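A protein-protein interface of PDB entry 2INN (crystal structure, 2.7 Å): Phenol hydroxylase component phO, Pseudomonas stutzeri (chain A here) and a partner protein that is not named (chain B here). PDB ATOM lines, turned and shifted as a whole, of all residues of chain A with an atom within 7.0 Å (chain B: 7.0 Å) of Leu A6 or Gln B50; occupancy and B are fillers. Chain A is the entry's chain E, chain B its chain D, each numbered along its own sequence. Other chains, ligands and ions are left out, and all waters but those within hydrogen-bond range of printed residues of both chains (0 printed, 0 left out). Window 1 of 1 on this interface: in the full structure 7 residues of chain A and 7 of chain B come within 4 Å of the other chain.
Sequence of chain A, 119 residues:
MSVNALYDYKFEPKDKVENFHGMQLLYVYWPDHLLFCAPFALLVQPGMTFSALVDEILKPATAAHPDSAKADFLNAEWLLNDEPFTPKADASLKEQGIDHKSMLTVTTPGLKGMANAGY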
ATOM      1  N   VAL A   3      18.029  -6.616  -1.392  1.00  0.00           N
ATOM      2  CA  VAL A   3      19.118  -7.395  -1.912  1.00  0.00           C
ATOM      3  C   VAL A   3      20.197  -6.569  -2.590  1.00  0.00           C
ATOM      4  O   VAL A   3      19.918  -5.834  -3.503  1.00  0.00           O
ATOM      5  CB  VAL A   3      18.508  -8.355  -2.985  1.00  0.00           C
ATOM      6  CG1 VAL A   3      19.446  -8.595  -4.175  1.00  0.00           C
ATOM      7  CG2 VAL A   3      18.101  -9.708  -2.364  1.00  0.00           C
ATOM      8  N   ASN A   4      21.455  -6.688  -2.267  1.00  0.00           N
ATOM      9  CA  ASN A   4      22.368  -6.115  -3.241  1.00  0.00           C
ATOM     10  C   ASN A   4      22.823  -7.121  -4.291  1.00  0.00           C
ATOM     11  O   ASN A   4      23.157  -8.264  -3.966  1.00  0.00           O
ATOM     12  CB  ASN A   4      23.551  -5.467  -2.561  1.00  0.00           C
ATOM     13  CG  ASN A   4      23.158  -4.184  -1.886  1.00  0.00           C
ATOM     14  OD1 ASN A   4      22.542  -4.198  -0.842  1.00  0.00           O
ATOM     15  ND2 ASN A   4      23.474  -3.056  -2.518  1.00  0.00           N
ATOM     16  N   ALA A   5      22.857  -6.705  -5.546  1.00  0.00           N
ATOM     17  CA  ALA A   5      23.124  -7.589  -6.620  1.00  0.00           C
ATOM     18  C   ALA A   5      23.854  -6.636  -7.445  1.00  0.00           C
ATOM     19  O   ALA A   5      23.844  -5.477  -7.133  1.00  0.00           O
ATOM     20  CB  ALA A   5      21.863  -7.908  -7.284  1.00  0.00           C
ATOM     21  N   LEU A   6      24.439  -7.136  -8.536  1.00  0.00           N
ATOM     22  CA  LEU A   6      25.207  -6.406  -9.547  1.00  0.00           C
ATOM     23  C   LEU A   6      24.380  -6.245 -10.904  1.00  0.00           C
ATOM     24  O   LEU A   6      24.863  -5.672 -11.910  1.00  0.00           O
ATOM     25  CB  LEU A   6      26.508  -7.219  -9.737  1.00  0.00           C
ATOM     26  CG  LEU A   6      27.882  -6.994 -10.362  1.00  0.00           C
ATOM     27  CD1 LEU A   6      28.558  -5.827  -9.696  1.00  0.00           C
ATOM     28  CD2 LEU A   6      28.698  -8.308 -10.174  1.00  0.00           C
ATOM     29  N   TYR A   7      23.129  -6.713 -10.924  1.00  0.00           N
ATOM     30  CA  TYR A   7      22.191  -6.395 -12.002  1.00  0.00           C
ATOM     31  C   TYR A   7      20.820  -6.185 -11.311  1.00  0.00           C
ATOM     32  O   TYR A   7      20.704  -6.236 -10.064  1.00  0.00           O
ATOM     33  CB  TYR A   7      22.139  -7.551 -12.963  1.00  0.00           C
ATOM     34  CG  TYR A   7      21.831  -8.906 -12.275  1.00  0.00           C
ATOM     35  CD1 TYR A   7      22.770  -9.569 -11.479  1.00  0.00           C
ATOM     36  CD2 TYR A   7      20.592  -9.523 -12.442  1.00  0.00           C
ATOM     37  CE1 TYR A   7      22.473 -10.824 -10.892  1.00  0.00           C
ATOM     38  CE2 TYR A   7      20.301 -10.763 -11.844  1.00  0.00           C
ATOM     39  CZ  TYR A   7      21.244 -11.419 -11.071  1.00  0.00           C
ATOM     40  OH  TYR A   7      20.886 -12.645 -10.484  1.00  0.00           O
ATOM     41  N   ASP A   8      19.758  -5.973 -12.087  1.00  0.00           N
ATOM     42  CA  ASP A   8      18.472  -5.711 -11.447  1.00  0.00           C
ATOM     43  C   ASP A   8      17.945  -7.025 -10.974  1.00  0.00           C
ATOM     44  O   ASP A   8      17.493  -7.778 -11.770  1.00  0.00           O
ATOM     45  CB  ASP A   8      17.522  -5.031 -12.444  1.00  0.00           C
ATOM     46  CG  ASP A   8      16.153  -4.689 -11.830  1.00  0.00           C
ATOM     47  OD1 ASP A   8      16.102  -4.340 -10.602  1.00  0.00           O
ATOM     48  OD2 ASP A   8      15.118  -4.775 -12.590  1.00  0.00           O
ATOM     49  N   TYR A   9      18.060  -7.305  -9.686  1.00  0.00           N
ATOM     50  CA  TYR A   9      17.776  -8.648  -9.142  1.00  0.00           C
ATOM     51  C   TYR A   9      16.285  -8.982  -9.015  1.00  0.00           C
ATOM     52  O   TYR A   9      15.639  -8.602  -8.048  1.00  0.00           O
ATOM     53  CB  TYR A   9      18.410  -8.734  -7.738  1.00  0.00           C
ATOM     54  CG  TYR A   9      18.721 -10.138  -7.236  1.00  0.00           C
ATOM     55  CD1 TYR A   9      19.860 -10.873  -7.742  1.00  0.00           C
ATOM     56  CD2 TYR A   9      17.895 -10.761  -6.278  1.00  0.00           C
ATOM     57  CE1 TYR A   9      20.157 -12.145  -7.291  1.00  0.00           C
ATOM     58  CE2 TYR A   9      18.189 -12.083  -5.831  1.00  0.00           C
ATOM     59  CZ  TYR A   9      19.339 -12.754  -6.335  1.00  0.00           C
ATOM     60  OH  TYR A   9      19.607 -14.038  -5.921  1.00  0.00           O
ATOM     61  N   PHE A  11      13.091 -11.911  -9.681  1.00  0.00           N
ATOM     62  CA  PHE A  11      12.800 -13.284 -10.109  1.00  0.00           C
ATOM     63  C   PHE A  11      11.321 -13.717  -9.796  1.00  0.00           C
ATOM     64  O   PHE A  11      10.783 -13.306  -8.751  1.00  0.00           O
ATOM     65  CB  PHE A  11      13.813 -14.278  -9.462  1.00  0.00           C
ATOM     66  CG  PHE A  11      15.268 -14.042  -9.875  1.00  0.00           C
ATOM     67  CD1 PHE A  11      15.770 -14.564 -11.065  1.00  0.00           C
ATOM     68  CD2 PHE A  11      16.122 -13.288  -9.086  1.00  0.00           C
ATOM     69  CE1 PHE A  11      17.098 -14.291 -11.505  1.00  0.00           C
ATOM     70  CE2 PHE A  11      17.453 -13.016  -9.523  1.00  0.00           C
ATOM     71  CZ  PHE A  11      17.935 -13.534 -10.729  1.00  0.00           C
ATOM     72  N   TYR B  47      19.051 -20.084  -4.910  1.00  0.00           N
ATOM     73  CA  TYR B  47      18.990 -18.664  -5.159  1.00  0.00           C
ATOM     74  C   TYR B  47      19.965 -18.416  -6.246  1.00  0.00           C
ATOM     75  O   TYR B  47      20.967 -19.124  -6.286  1.00  0.00           O
ATOM     76  CB  TYR B  47      19.432 -17.902  -3.946  1.00  0.00           C
ATOM     77  CG  TYR B  47      19.014 -18.524  -2.628  1.00  0.00           C
ATOM     78  CD1 TYR B  47      19.941 -19.283  -1.853  1.00  0.00           C
ATOM     79  CD2 TYR B  47      17.714 -18.336  -2.099  1.00  0.00           C
ATOM     80  CE1 TYR B  47      19.585 -19.810  -0.645  1.00  0.00           C
ATOM     81  CE2 TYR B  47      17.353 -18.881  -0.882  1.00  0.00           C
ATOM     82  CZ  TYR B  47      18.305 -19.597  -0.142  1.00  0.00           C
ATOM     83  OH  TYR B  47      17.960 -20.167   1.098  1.00  0.00           O
ATOM     84  N   ARG B  48      19.704 -17.488  -7.159  1.00  0.00           N
ATOM     85  CA  ARG B  48      20.643 -17.251  -8.269  1.00  0.00           C
ATOM     86  C   ARG B  48      21.780 -16.373  -7.795  1.00  0.00           C
ATOM     87  O   ARG B  48      21.617 -15.596  -6.916  1.00  0.00           O
ATOM     88  CB  ARG B  48      19.933 -16.528  -9.437  1.00  0.00           C
ATOM     89  CG  ARG B  48      18.765 -17.313  -9.921  1.00  0.00           C
ATOM     90  CD  ARG B  48      19.206 -18.228 -10.975  1.00  0.00           C
ATOM     91  NE  ARG B  48      19.751 -17.297 -11.936  1.00  0.00           N
ATOM     92  CZ  ARG B  48      19.453 -17.322 -13.217  1.00  0.00           C
ATOM     93  NH1 ARG B  48      19.991 -16.413 -13.977  1.00  0.00           N
ATOM     94  NH2 ARG B  48      18.665 -18.272 -13.719  1.00  0.00           N
ATOM     95  N   PRO B  49      22.941 -16.513  -8.382  1.00  0.00           N
ATOM     96  CA  PRO B  49      24.019 -15.629  -8.046  1.00  0.00           C
ATOM     97  C   PRO B  49      23.701 -14.142  -8.129  1.00  0.00           C
ATOM     98  O   PRO B  49      23.287 -13.614  -9.185  1.00  0.00           O
ATOM     99  CB  PRO B  49      25.107 -15.988  -9.066  1.00  0.00           C
ATOM    100  CG  PRO B  49      24.653 -17.158  -9.779  1.00  0.00           C
ATOM    101  CD  PRO B  49      23.357 -17.595  -9.268  1.00  0.00           C
ATOM    102  N   GLN B  50      24.024 -13.434  -7.049  1.00  0.00           N
ATOM    103  CA  GLN B  50      23.881 -11.962  -7.084  1.00  0.00           C
ATOM    104  C   GLN B  50      24.955 -11.324  -7.894  1.00  0.00           C
ATOM    105  O   GLN B  50      24.865 -10.154  -8.194  1.00  0.00           O
ATOM    106  CB  GLN B  50      23.772 -11.364  -5.693  1.00  0.00           C
ATOM    107  CG  GLN B  50      22.644 -12.027  -4.906  1.00  0.00           C
ATOM    108  CD  GLN B  50      22.816 -11.896  -3.422  1.00  0.00           C
ATOM    109  OE1 GLN B  50      23.092 -10.794  -2.908  1.00  0.00           O
ATOM    110  NE2 GLN B  50      22.585 -12.998  -2.691  1.00  0.00           N
ATOM    111  N   TRP B  51      25.966 -12.078  -8.297  1.00  0.00           N
ATOM    112  CA  TRP B  51      27.160 -11.472  -8.894  1.00  0.00           C
ATOM    113  C   TRP B  51      27.285 -11.940 -10.358  1.00  0.00           C
ATOM    114  O   TRP B  51      28.334 -11.756 -11.000  1.00  0.00           O
ATOM    115  CB  TRP B  51      28.402 -11.748  -7.983  1.00  0.00           C
ATOM    116  CG  TRP B  51      28.310 -13.113  -7.472  1.00  0.00           C
ATOM    117  CD1 TRP B  51      27.807 -13.507  -6.271  1.00  0.00           C
ATOM    118  CD2 TRP B  51      28.616 -14.288  -8.189  1.00  0.00           C
ATOM    119  NE1 TRP B  51      27.765 -14.865  -6.179  1.00  0.00           N
ATOM    120  CE2 TRP B  51      28.284 -15.389  -7.336  1.00  0.00           C
ATOM    121  CE3 TRP B  51      29.130 -14.541  -9.490  1.00  0.00           C
ATOM    122  CZ2 TRP B  51      28.437 -16.749  -7.750  1.00  0.00           C
ATOM    123  CZ3 TRP B  51      29.268 -15.865  -9.918  1.00  0.00           C
ATOM    124  CH2 TRP B  51      28.930 -16.969  -9.028  1.00  0.00           C
ATOM    125  N   ASP B  52      26.200 -12.524 -10.897  1.00  0.00           N
ATOM    126  CA  ASP B  52      26.156 -13.024 -12.303  1.00  0.00           C
ATOM    127  C   ASP B  52      24.687 -13.107 -12.767  1.00  0.00           C
ATOM    128  O   ASP B  52      23.901 -13.782 -12.155  1.00  0.00           O
ATOM    129  CB  ASP B  52      26.885 -14.362 -12.405  1.00  0.00           C
ATOM    130  CG  ASP B  52      26.851 -15.023 -13.850  1.00  0.00           C
ATOM    131  OD1 ASP B  52      26.362 -14.392 -14.840  1.00  0.00           O
ATOM    132  OD2 ASP B  52      27.330 -16.218 -13.977  1.00  0.00           O
ATOM    133  N   SER B  53      24.284 -12.375 -13.805  1.00  0.00           N
ATOM    134  CA  SER B  53      22.868 -12.533 -14.232  1.00  0.00           C
ATOM    135  C   SER B  53      22.755 -13.628 -15.212  1.00  0.00           C
ATOM    136  O   SER B  53      21.653 -13.979 -15.557  1.00  0.00           O
ATOM    137  CB  SER B  53      22.289 -11.311 -14.952  1.00  0.00           C
ATOM    138  OG  SER B  53      23.327 -10.658 -15.621  1.00  0.00           O
ATOM    139  N   LEU B  57      24.416 -20.954  -9.862  1.00  0.00           N
ATOM    140  CA  LEU B  57      25.513 -21.509  -9.178  1.00  0.00           C
ATOM    141  C   LEU B  57      25.881 -22.819  -9.987  1.00  0.00           C
ATOM    142  O   LEU B  57      24.961 -23.502 -10.500  1.00  0.00           O
ATOM    143  CB  LEU B  57      24.982 -21.827  -7.821  1.00  0.00           C
ATOM    144  CG  LEU B  57      25.370 -21.053  -6.578  1.00  0.00           C
ATOM    145  CD1 LEU B  57      25.991 -19.643  -6.795  1.00  0.00           C
ATOM    146  CD2 LEU B  57      24.348 -21.059  -5.520  1.00  0.00           C
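The guanidinium group of Arg B48 sits at hydrogen-bond distance from the backbone carbonyl oxygen of Ser B53, 3.3 Å away.
O of Gln B50 touches CA of Ala A5, 3.5 Å away. CD2 of Leu A6 touches O of Trp B51 (3.6 Å). CE1 of Tyr A7 touches O of Gln B50, at 3.7 Å. Asp B52 touches Tyr A7 (O to CE1, 3.5 Å). Tyr A7 touches Ser B53 (CD2 to CB, 3.5 Å). Tyr A9 touches Pro B49 (CE1 to O, 3.9 Å). CE1 of Tyr A9 touches CG of Gln B50, at 3.4 Å. Phe A11 touches Arg B48 (CE1 to CG, 3.8 Å).
Printed residues of chain B that touch a printed residue of chain A: Arg B48, Pro B49, Gln B50, Trp B51, Asp B52 and Ser B53. Hydrophobic or aromatic side chains of chain A that line the printed part of chain B: Ala A5, Leu A6, Tyr A7, Tyr A9 and Phe A11. Among the printed residues, 12 pairs touch across the chains. Among the printed residues, no Asp or Glu carboxylate lies within 4 Å of a Lys or Arg side-chain nitrogen of the other chain.
Of the printed residues of chain B, Ala A5 touches Gln B50. Leu A6 touches just these residues of chain B: Gln B50 and Trp B51. Asp A8 touches none of the printed residues of chain B. Gln B50 touches just these residues of chain A: Asn A4, Ala A5, Leu A6, Tyr A7 and Tyr A9. Of the printed residues of chain A, Asp B52 touches Tyr A7. Of the printed residues of chain A, Ser B53 touches Tyr A7 (3.5 Å). Leu B57 touches none of the printed residues of chain A. The nearest printed residue of chain A that does not touch Arg B48 is Tyr A7 (4.1 Å).
OE1 of Gln B50 sits close to O of Asn A4 (2.7 Å). The side-chain hydroxyl (OH) of Tyr A9 sits at hydrogen-bond distance from the backbone carbonyl oxygen (O) of Arg B48. The backbone carbonyl oxygen (O) of Pro B49 lies within hydrogen-bond range of the side-chain hydroxyl (OH) of Tyr A7, 2.9 Å away. The backbone carbonyl oxygen of Gln B50 sits at hydrogen-bond distance from the backbone NH of Leu A6.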
